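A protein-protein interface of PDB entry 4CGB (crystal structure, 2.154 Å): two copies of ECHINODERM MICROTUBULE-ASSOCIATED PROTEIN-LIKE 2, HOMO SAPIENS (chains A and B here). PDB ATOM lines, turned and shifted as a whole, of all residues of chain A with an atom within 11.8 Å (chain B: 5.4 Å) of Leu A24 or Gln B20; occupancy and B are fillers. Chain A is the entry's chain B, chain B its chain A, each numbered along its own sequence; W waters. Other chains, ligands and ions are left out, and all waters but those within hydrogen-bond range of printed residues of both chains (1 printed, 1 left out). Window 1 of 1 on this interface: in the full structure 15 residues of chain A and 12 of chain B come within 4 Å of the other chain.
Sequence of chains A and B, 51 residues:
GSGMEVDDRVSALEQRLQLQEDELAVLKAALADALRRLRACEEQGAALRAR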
ATOM      1  N   ALA A  12      15.545  -0.201  32.157  1.00  0.00           N
ATOM      2  CA  ALA A  12      16.921  -0.135  32.642  1.00  0.00           C
ATOM      3  C   ALA A  12      17.914  -0.334  31.494  1.00  0.00           C
ATOM      4  O   ALA A  12      18.986   0.276  31.482  1.00  0.00           O
ATOM      5  CB  ALA A  12      17.157  -1.158  33.755  1.00  0.00           C
ATOM      6  N   LEU A  13      17.547  -1.169  30.525  1.00  0.00           N
ATOM      7  CA  LEU A  13      18.363  -1.364  29.327  1.00  0.00           C
ATOM      8  C   LEU A  13      18.443  -0.095  28.482  1.00  0.00           C
ATOM      9  O   LEU A  13      19.514   0.270  27.994  1.00  0.00           O
ATOM     10  CB  LEU A  13      17.807  -2.505  28.470  1.00  0.00           C
ATOM     11  CG  LEU A  13      18.225  -3.932  28.821  1.00  0.00           C
ATOM     12  CD1 LEU A  13      17.503  -4.941  27.924  1.00  0.00           C
ATOM     13  CD2 LEU A  13      19.728  -4.084  28.690  1.00  0.00           C
ATOM     14  N   GLU A  14      17.299   0.563  28.303  1.00  0.00           N
ATOM     15  CA  GLU A  14      17.220   1.779  27.501  1.00  0.00           C
ATOM     16  C   GLU A  14      18.057   2.903  28.110  1.00  0.00           C
ATOM     17  O   GLU A  14      18.649   3.707  27.387  1.00  0.00           O
ATOM     18  CB  GLU A  14      15.762   2.217  27.333  1.00  0.00           C
ATOM     19  CG  GLU A  14      14.960   1.322  26.391  1.00  0.00           C
ATOM     20  CD  GLU A  14      13.460   1.478  26.554  1.00  0.00           C
ATOM     21  OE1 GLU A  14      13.013   1.865  27.656  1.00  0.00           O
ATOM     22  OE2 GLU A  14      12.724   1.212  25.579  1.00  0.00           O
ATOM     23  N   GLN A  15      18.109   2.945  29.437  1.00  0.00           N
ATOM     24  CA  GLN A  15      18.937   3.920  30.141  1.00  0.00           C
ATOM     25  C   GLN A  15      20.423   3.649  29.903  1.00  0.00           C
ATOM     26  O   GLN A  15      21.179   4.559  29.561  1.00  0.00           O
ATOM     27  CB  GLN A  15      18.625   3.905  31.641  1.00  0.00           C
ATOM     28  N   ARG A  16      20.833   2.394  30.079  1.00  0.00           N
ATOM     29  CA  ARG A  16      22.218   2.003  29.826  1.00  0.00           C
ATOM     30  C   ARG A  16      22.628   2.217  28.372  1.00  0.00           C
ATOM     31  O   ARG A  16      23.785   2.510  28.088  1.00  0.00           O
ATOM     32  CB  ARG A  16      22.470   0.551  30.235  1.00  0.00           C
ATOM     33  CG  ARG A  16      22.675   0.369  31.723  1.00  0.00           C
ATOM     34  CD  ARG A  16      22.722  -1.096  32.087  1.00  0.00           C
ATOM     35  NE  ARG A  16      23.918  -1.787  31.616  1.00  0.00           N
ATOM     36  CZ  ARG A  16      23.997  -3.109  31.475  1.00  0.00           C
ATOM     37  NH1 ARG A  16      22.945  -3.878  31.747  1.00  0.00           N
ATOM     38  NH2 ARG A  16      25.123  -3.665  31.048  1.00  0.00           N
ATOM     39  N   LEU A  17      21.680   2.074  27.451  1.00  0.00           N
ATOM     40  CA  LEU A  17      21.985   2.271  26.041  1.00  0.00           C
ATOM     41  C   LEU A  17      22.158   3.752  25.716  1.00  0.00           C
ATOM     42  O   LEU A  17      23.030   4.118  24.917  1.00  0.00           O
ATOM     43  CB  LEU A  17      20.913   1.648  25.150  1.00  0.00           C
ATOM     44  CG  LEU A  17      21.429   0.971  23.885  1.00  0.00           C
ATOM     45  CD1 LEU A  17      22.720   0.231  24.172  1.00  0.00           C
ATOM     46  CD2 LEU A  17      20.384   0.005  23.378  1.00  0.00           C
ATOM     47  N   GLN A  18      21.336   4.599  26.333  1.00  0.00           N
ATOM     48  CA  GLN A  18      21.486   6.045  26.174  1.00  0.00           C
ATOM     49  C   GLN A  18      22.842   6.532  26.678  1.00  0.00           C
ATOM     50  O   GLN A  18      23.483   7.380  26.047  1.00  0.00           O
ATOM     51  CB  GLN A  18      20.368   6.816  26.885  1.00  0.00           C
ATOM     52  CG  GLN A  18      20.534   8.329  26.783  1.00  0.00           C
ATOM     53  CD  GLN A  18      20.650   8.804  25.341  1.00  0.00           C
ATOM     54  OE1 GLN A  18      21.655   9.404  24.945  1.00  0.00           O
ATOM     55  NE2 GLN A  18      19.616   8.540  24.549  1.00  0.00           N
ATOM     56  N   LEU A  19      23.286   5.997  27.809  1.00  0.00           N
ATOM     57  CA  LEU A  19      24.577   6.401  28.361  1.00  0.00           C
ATOM     58  C   LEU A  19      25.736   5.939  27.480  1.00  0.00           C
ATOM     59  O   LEU A  19      26.737   6.643  27.338  1.00  0.00           O
ATOM     60  CB  LEU A  19      24.736   5.889  29.788  1.00  0.00           C
ATOM     61  CG  LEU A  19      23.745   6.604  30.708  1.00  0.00           C
ATOM     62  CD1 LEU A  19      23.604   5.879  32.035  1.00  0.00           C
ATOM     63  CD2 LEU A  19      24.170   8.064  30.910  1.00  0.00           C
ATOM     64  N   GLN A  20      25.583   4.762  26.886  1.00  0.00           N
ATOM     65  CA  GLN A  20      26.566   4.250  25.944  1.00  0.00           C
ATOM     66  C   GLN A  20      26.646   5.165  24.735  1.00  0.00           C
ATOM     67  O   GLN A  20      27.731   5.428  24.214  1.00  0.00           O
ATOM     68  CB  GLN A  20      26.203   2.828  25.517  1.00  0.00           C
ATOM     69  CG  GLN A  20      26.754   1.764  26.440  1.00  0.00           C
ATOM     70  CD  GLN A  20      28.259   1.646  26.324  1.00  0.00           C
ATOM     71  OE1 GLN A  20      28.999   2.109  27.192  1.00  0.00           O
ATOM     72  NE2 GLN A  20      28.721   1.022  25.244  1.00  0.00           N
ATOM     73  N   GLU A  21      25.488   5.661  24.310  1.00  0.00           N
ATOM     74  CA  GLU A  21      25.401   6.555  23.161  1.00  0.00           C
ATOM     75  C   GLU A  21      26.136   7.867  23.426  1.00  0.00           C
ATOM     76  O   GLU A  21      26.835   8.383  22.555  1.00  0.00           O
ATOM     77  CB  GLU A  21      23.941   6.846  22.844  1.00  0.00           C
ATOM     78  CG  GLU A  21      23.581   6.726  21.380  1.00  0.00           C
ATOM     79  CD  GLU A  21      22.146   6.273  21.185  1.00  0.00           C
ATOM     80  OE1 GLU A  21      21.257   6.753  21.921  1.00  0.00           O
ATOM     81  OE2 GLU A  21      21.913   5.417  20.305  1.00  0.00           O
ATOM     82  N   ASP A  22      25.955   8.402  24.623  1.00  0.00           N
ATOM     83  CA  ASP A  22      26.651   9.612  25.040  1.00  0.00           C
ATOM     84  C   ASP A  22      28.157   9.397  25.008  1.00  0.00           C
ATOM     85  O   ASP A  22      28.903  10.224  24.466  1.00  0.00           O
ATOM     86  CB  ASP A  22      26.231  10.004  26.454  1.00  0.00           C
ATOM     87  CG  ASP A  22      24.901  10.725  26.493  1.00  0.00           C
ATOM     88  OD1 ASP A  22      24.202  10.733  25.459  1.00  0.00           O
ATOM     89  OD2 ASP A  22      24.554  11.280  27.562  1.00  0.00           O
ATOM     90  N   GLU A  23      28.600   8.290  25.606  1.00  0.00           N
ATOM     91  CA  GLU A  23      30.022   7.962  25.678  1.00  0.00           C
ATOM     92  C   GLU A  23      30.633   7.815  24.289  1.00  0.00           C
ATOM     93  O   GLU A  23      31.728   8.298  24.041  1.00  0.00           O
ATOM     94  CB  GLU A  23      30.251   6.674  26.478  1.00  0.00           C
ATOM     95  CG  GLU A  23      29.819   6.727  27.953  1.00  0.00           C
ATOM     96  CD  GLU A  23      30.893   7.275  28.888  1.00  0.00           C
ATOM     97  OE1 GLU A  23      32.047   7.458  28.447  1.00  0.00           O
ATOM     98  OE2 GLU A  23      30.578   7.518  30.073  1.00  0.00           O
ATOM     99  N   LEU A  24      29.923   7.143  23.383  1.00  0.00           N
ATOM    100  CA  LEU A  24      30.438   6.961  22.038  1.00  0.00           C
ATOM    101  C   LEU A  24      30.568   8.289  21.303  1.00  0.00           C
ATOM    102  O   LEU A  24      31.561   8.519  20.622  1.00  0.00           O
ATOM    103  CB  LEU A  24      29.572   5.987  21.243  1.00  0.00           C
ATOM    104  CG  LEU A  24      29.617   4.563  21.787  1.00  0.00           C
ATOM    105  CD1 LEU A  24      28.363   3.794  21.368  1.00  0.00           C
ATOM    106  CD2 LEU A  24      30.878   3.857  21.313  1.00  0.00           C
ATOM    107  N   ALA A  25      29.577   9.164  21.446  1.00  0.00           N
ATOM    108  CA  ALA A  25      29.648  10.475  20.812  1.00  0.00           C
ATOM    109  C   ALA A  25      30.897  11.230  21.271  1.00  0.00           C
ATOM    110  O   ALA A  25      31.615  11.817  20.460  1.00  0.00           O
ATOM    111  CB  ALA A  25      28.395  11.287  21.113  1.00  0.00           C
ATOM    112  N   VAL A  26      31.155  11.187  22.569  1.00  0.00           N
ATOM    113  CA  VAL A  26      32.273  11.912  23.171  1.00  0.00           C
ATOM    114  C   VAL A  26      33.626  11.323  22.756  1.00  0.00           C
ATOM    115  O   VAL A  26      34.551  12.060  22.409  1.00  0.00           O
ATOM    116  CB  VAL A  26      32.138  11.953  24.721  1.00  0.00           C
ATOM    117  CG1 VAL A  26      33.463  12.260  25.373  1.00  0.00           C
ATOM    118  CG2 VAL A  26      31.085  12.973  25.136  1.00  0.00           C
ATOM    119  N   LEU A  27      33.721   9.997  22.770  1.00  0.00           N
ATOM    120  CA  LEU A  27      34.947   9.292  22.400  1.00  0.00           C
ATOM    121  C   LEU A  27      35.302   9.474  20.927  1.00  0.00           C
ATOM    122  O   LEU A  27      36.474   9.591  20.574  1.00  0.00           O
ATOM    123  CB  LEU A  27      34.820   7.807  22.737  1.00  0.00           C
ATOM    124  CG  LEU A  27      34.876   7.526  24.239  1.00  0.00           C
ATOM    125  CD1 LEU A  27      34.552   6.073  24.517  1.00  0.00           C
ATOM    126  CD2 LEU A  27      36.241   7.885  24.814  1.00  0.00           C
ATOM    127  N   LYS A  28      34.278   9.495  20.080  1.00  0.00           N
ATOM    128  CA  LYS A  28      34.439   9.766  18.657  1.00  0.00           C
ATOM    129  C   LYS A  28      34.983  11.170  18.374  1.00  0.00           C
ATOM    130  O   LYS A  28      35.892  11.331  17.556  1.00  0.00           O
ATOM    131  CB  LYS A  28      33.105   9.553  17.937  1.00  0.00           C
ATOM    132  CG  LYS A  28      33.066  10.043  16.500  1.00  0.00           C
ATOM    133  CD  LYS A  28      31.670   9.857  15.911  1.00  0.00           C
ATOM    134  CE  LYS A  28      31.233   8.400  15.977  1.00  0.00           C
ATOM    135  NZ  LYS A  28      29.746   8.251  15.964  1.00  0.00           N
ATOM    136  N   ALA A  29      34.429  12.186  19.038  1.00  0.00           N
ATOM    137  CA  ALA A  29      34.965  13.541  18.911  1.00  0.00           C
ATOM    138  C   ALA A  29      36.383  13.619  19.472  1.00  0.00           C
ATOM    139  O   ALA A  29      37.235  14.323  18.924  1.00  0.00           O
ATOM    140  CB  ALA A  29      34.055  14.564  19.602  1.00  0.00           C
ATOM    141  N   ALA A  30      36.639  12.891  20.558  1.00  0.00           N
ATOM    142  CA  ALA A  30      37.964  12.891  21.182  1.00  0.00           C
ATOM    143  C   ALA A  30      39.003  12.191  20.303  1.00  0.00           C
ATOM    144  O   ALA A  30      40.162  12.594  20.265  1.00  0.00           O
ATOM    145  CB  ALA A  30      37.906  12.235  22.558  1.00  0.00           C
ATOM    146  N   LEU A  31      38.587  11.138  19.616  1.00  0.00           N
ATOM    147  CA  LEU A  31      39.466  10.435  18.693  1.00  0.00           C
ATOM    148  C   LEU A  31      39.840  11.325  17.512  1.00  0.00           C
ATOM    149  O   LEU A  31      41.013  11.399  17.125  1.00  0.00           O
ATOM    150  CB  LEU A  31      38.807   9.141  18.201  1.00  0.00           C
ATOM    151  CG  LEU A  31      39.653   8.293  17.235  1.00  0.00           C
ATOM    152  CD1 LEU A  31      40.929   7.810  17.907  1.00  0.00           C
ATOM    153  CD2 LEU A  31      38.853   7.120  16.697  1.00  0.00           C
ATOM    154  N   ALA A  32      38.842  11.993  16.942  1.00  0.00           N
ATOM    155  CA  ALA A  32      39.075  12.967  15.879  1.00  0.00           C
ATOM    156  C   ALA A  32      40.129  13.996  16.288  1.00  0.00           C
ATOM    157  O   ALA A  32      41.046  14.293  15.525  1.00  0.00           O
ATOM    158  CB  ALA A  32      37.774  13.658  15.493  1.00  0.00           C
ATOM    159  N   ASP A  33      40.010  14.528  17.502  1.00  0.00           N
ATOM    160  CA  ASP A  33      41.025  15.451  18.006  1.00  0.00           C
ATOM    161  C   ASP A  33      42.395  14.778  18.134  1.00  0.00           C
ATOM    162  O   ASP A  33      43.417  15.384  17.816  1.00  0.00           O
ATOM    163  CB  ASP A  33      40.613  16.053  19.349  1.00  0.00           C
ATOM    164  CG  ASP A  33      41.535  17.187  19.782  1.00  0.00           C
ATOM    165  OD1 ASP A  33      41.439  18.286  19.190  1.00  0.00           O
ATOM    166  OD2 ASP A  33      42.349  16.981  20.708  1.00  0.00           O
ATOM    167  N   ARG B  16      19.572  -1.121  18.014  1.00  0.00           N
ATOM    168  CA  ARG B  16      20.405  -0.032  18.502  1.00  0.00           C
ATOM    169  C   ARG B  16      21.740  -0.537  19.020  1.00  0.00           C
ATOM    170  O   ARG B  16      22.777   0.089  18.790  1.00  0.00           O
ATOM    171  CB  ARG B  16      19.695   0.742  19.613  1.00  0.00           C
ATOM    172  CG  ARG B  16      18.645   1.718  19.121  1.00  0.00           C
ATOM    173  CD  ARG B  16      17.940   2.392  20.281  1.00  0.00           C
ATOM    174  NE  ARG B  16      18.811   3.312  21.005  1.00  0.00           N
ATOM    175  CZ  ARG B  16      18.510   3.843  22.188  1.00  0.00           C
ATOM    176  NH1 ARG B  16      17.369   3.529  22.789  1.00  0.00           N
ATOM    177  NH2 ARG B  16      19.358   4.673  22.780  1.00  0.00           N
ATOM    178  N   LEU B  17      21.715  -1.662  19.730  1.00  0.00           N
ATOM    179  CA  LEU B  17      22.944  -2.230  20.271  1.00  0.00           C
ATOM    180  C   LEU B  17      23.938  -2.587  19.159  1.00  0.00           C
ATOM    181  O   LEU B  17      25.135  -2.335  19.293  1.00  0.00           O
ATOM    182  CB  LEU B  17      22.656  -3.439  21.173  1.00  0.00           C
ATOM    183  CG  LEU B  17      23.890  -4.104  21.802  1.00  0.00           C
ATOM    184  CD1 LEU B  17      24.804  -3.072  22.458  1.00  0.00           C
ATOM    185  CD2 LEU B  17      23.493  -5.175  22.808  1.00  0.00           C
ATOM    186  N   GLN B  18      23.435  -3.145  18.053  1.00  0.00           N
ATOM    187  CA  GLN B  18      24.307  -3.495  16.933  1.00  0.00           C
ATOM    188  C   GLN B  18      24.899  -2.274  16.221  1.00  0.00           C
ATOM    189  O   GLN B  18      26.049  -2.307  15.803  1.00  0.00           O
ATOM    190  CB  GLN B  18      23.628  -4.469  15.952  1.00  0.00           C
ATOM    191  CG  GLN B  18      22.274  -4.018  15.426  1.00  0.00           C
ATOM    192  CD  GLN B  18      21.607  -5.048  14.514  1.00  0.00           C
ATOM    193  OE1 GLN B  18      21.557  -6.245  14.829  1.00  0.00           O
ATOM    194  NE2 GLN B  18      21.092  -4.580  13.377  1.00  0.00           N
ATOM    195  N   LEU B  19      24.133  -1.198  16.099  1.00  0.00           N
ATOM    196  CA  LEU B  19      24.675   0.046  15.548  1.00  0.00           C
ATOM    197  C   LEU B  19      25.766   0.628  16.450  1.00  0.00           C
ATOM    198  O   LEU B  19      26.773   1.143  15.959  1.00  0.00           O
ATOM    199  CB  LEU B  19      23.569   1.078  15.319  1.00  0.00           C
ATOM    200  CG  LEU B  19      22.546   0.742  14.226  1.00  0.00           C
ATOM    201  CD1 LEU B  19      21.598   1.914  14.014  1.00  0.00           C
ATOM    202  CD2 LEU B  19      23.253   0.367  12.926  1.00  0.00           C
ATOM    203  N   GLN B  20      25.577   0.532  17.762  1.00  0.00           N
ATOM    204  CA  GLN B  20      26.603   0.971  18.705  1.00  0.00           C
ATOM    205  C   GLN B  20      27.851   0.094  18.625  1.00  0.00           C
ATOM    206  O   GLN B  20      28.967   0.602  18.726  1.00  0.00           O
ATOM    207  CB  GLN B  20      26.062   1.008  20.130  1.00  0.00           C
ATOM    208  CG  GLN B  20      24.940   2.003  20.314  1.00  0.00           C
ATOM    209  CD  GLN B  20      24.634   2.254  21.773  1.00  0.00           C
ATOM    210  OE1 GLN B  20      25.206   1.613  22.655  1.00  0.00           O
ATOM    211  NE2 GLN B  20      23.735   3.195  22.036  1.00  0.00           N
ATOM    212  N   GLU B  21      27.657  -1.213  18.443  1.00  0.00           N
ATOM    213  CA  GLU B  21      28.763  -2.143  18.206  1.00  0.00           C
ATOM    214  C   GLU B  21      29.603  -1.675  17.030  1.00  0.00           C
ATOM    215  O   GLU B  21      30.832  -1.729  17.056  1.00  0.00           O
ATOM    216  CB  GLU B  21      28.233  -3.538  17.875  1.00  0.00           C
ATOM    217  CG  GLU B  21      28.292  -4.551  19.002  1.00  0.00           C
ATOM    218  CD  GLU B  21      27.831  -5.935  18.557  1.00  0.00           C
ATOM    219  OE1 GLU B  21      28.372  -6.461  17.556  1.00  0.00           O
ATOM    220  OE2 GLU B  21      26.921  -6.493  19.207  1.00  0.00           O
ATOM    221  N   ASP B  22      28.926  -1.219  15.983  1.00  0.00           N
ATOM    222  CA  ASP B  22      29.612  -0.842  14.760  1.00  0.00           C
ATOM    223  C   ASP B  22      30.397   0.464  14.939  1.00  0.00           C
ATOM    224  O   ASP B  22      31.530   0.593  14.451  1.00  0.00           O
ATOM    225  CB  ASP B  22      28.614  -0.766  13.608  1.00  0.00           C
ATOM    226  CG  ASP B  22      27.877  -2.091  13.386  1.00  0.00           C
ATOM    227  OD1 ASP B  22      28.486  -3.167  13.573  1.00  0.00           O
ATOM    228  OD2 ASP B  22      26.682  -2.056  13.014  1.00  0.00           O
ATOM    229  N   GLU B  23      29.798   1.417  15.655  1.00  0.00           N
ATOM    230  CA  GLU B  23      30.475   2.643  16.048  1.00  0.00           C
ATOM    231  C   GLU B  23      31.749   2.338  16.828  1.00  0.00           C
ATOM    232  O   GLU B  23      32.816   2.860  16.510  1.00  0.00           O
ATOM    233  CB  GLU B  23      29.552   3.508  16.904  1.00  0.00           C
ATOM    234  CG  GLU B  23      28.300   3.982  16.195  1.00  0.00           C
ATOM    235  CD  GLU B  23      28.600   5.012  15.132  1.00  0.00           C
ATOM    236  OE1 GLU B  23      29.582   5.767  15.301  1.00  0.00           O
ATOM    237  OE2 GLU B  23      27.862   5.067  14.124  1.00  0.00           O
ATOM    238  N   LEU B  24      31.639   1.489  17.845  1.00  0.00           N
ATOM    239  CA  LEU B  24      32.793   1.150  18.675  1.00  0.00           C
ATOM    240  C   LEU B  24      33.893   0.480  17.855  1.00  0.00           C
ATOM    241  O   LEU B  24      35.073   0.701  18.105  1.00  0.00           O
ATOM    242  CB  LEU B  24      32.378   0.274  19.862  1.00  0.00           C
ATOM    243  CG  LEU B  24      33.430  -0.070  20.917  1.00  0.00           C
ATOM    244  CD1 LEU B  24      34.328   1.120  21.229  1.00  0.00           C
ATOM    245  CD2 LEU B  24      32.755  -0.544  22.190  1.00  0.00           C
ATOM    246  N   ALA B  25      33.498  -0.320  16.868  1.00  0.00           N
ATOM    247  CA  ALA B  25      34.455  -0.994  15.991  1.00  0.00           C
ATOM    248  C   ALA B  25      35.309  -0.015  15.184  1.00  0.00           C
ATOM    249  O   ALA B  25      36.512  -0.221  15.033  1.00  0.00           O
ATOM    250  CB  ALA B  25      33.728  -1.952  15.048  1.00  0.00           C
ATOM    251  N   LEU B  27      35.867   3.167  16.020  1.00  0.00           N
ATOM    252  CA  LEU B  27      36.682   3.826  17.031  1.00  0.00           C
ATOM    253  C   LEU B  27      37.897   2.983  17.428  1.00  0.00           C
ATOM    254  O   LEU B  27      39.016   3.471  17.466  1.00  0.00           O
ATOM    255  CB  LEU B  27      35.832   4.162  18.262  1.00  0.00           C
ATOM    256  CG  LEU B  27      35.302   5.600  18.366  1.00  0.00           C
ATOM    257  CD1 LEU B  27      34.934   6.174  17.001  1.00  0.00           C
ATOM    258  CD2 LEU B  27      34.108   5.679  19.313  1.00  0.00           C
HETATM  259  O   HOH W   1      22.407   3.260  18.317  1.00  0.00           O
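Leu A17 touches Arg B16, but with the chains exchanged Arg A16 does not touch Leu B17 (8.0 Å). Leu A17 touches Gln B20, but with the chains exchanged Gln A20 does not touch Leu B17 (6.3 Å). Gln A20 touches its own counterpart, Gln B20. Glu A21 touches Arg B16, but with the chains exchanged Arg A16 does not touch Glu B21 (11.0 Å). Of the 9 pairs that touch across the chains among the printed residues, 1 has its exchanged pair printed and touching as well.
Water W1 lies within hydrogen-bond range of OE2 of Glu A21 (3.0 Å) and O of Arg B16 (3.2 Å).
Of the 11 printed residues of chain B, 4 touch a printed residue of chain A. Hydrophobic or aromatic side chains of chain B within 4 Å of the printed part of chain A: Leu B27.
The guanidinium group (NH2) of Arg B16 is in salt-bridge range of the side-chain carboxylate (OE1) of Glu A21, 2.9 Å away. O of Leu A17 lies within hydrogen-bond range of NE2 of Gln B20, at 3.1 Å. NE2 of Gln B20 is in hydrogen-bond range of OE2 of Glu A21. OE1 of Glu B23 is in salt-bridge range of NZ of Lys A28 (2.6 Å).
Of the printed residues of chain B, Leu A17 touches Arg B16 and Gln B20. Leu A24 touches just one residue of chain B: Gln B20 (3.8 Å). Val A26 touches none of the printed residues of chain B. Printed residues of chain B within 4 Å of Lys A28: Glu B23 and Leu B27. Arg B16 touches just these residues of chain A: Leu A17 (3.9 Å) and Glu A21 (2.9 Å). No residue of chain A comes within 4 Å of Leu B17. No residue of chain A comes within 4 Å of Leu B19. Of chain A, only Leu A17 (3.1 Å), Gln A20 (3.3 Å), Glu A21 (3.4 Å) and Leu A24 (3.8 Å) come within 4 Å of Gln B20. Glu B21 touches none of the printed residues of chain A. Asp B22 touches none of the printed residues of chain A. Glu B23 touches one residue of chain A. Leu B24 touches none of the printed residues of chain A.
Among the printed residues, merely in contact across the chains: Leu A17 with Arg B16 (3.9 Å), Gln A20 with Gln B20 (3.3 Å), Leu A24 with Gln B20 (3.8 Å), Lys A28 with Leu B27 (3.9 Å) and Leu A31 with Leu B27 (3.7 Å).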
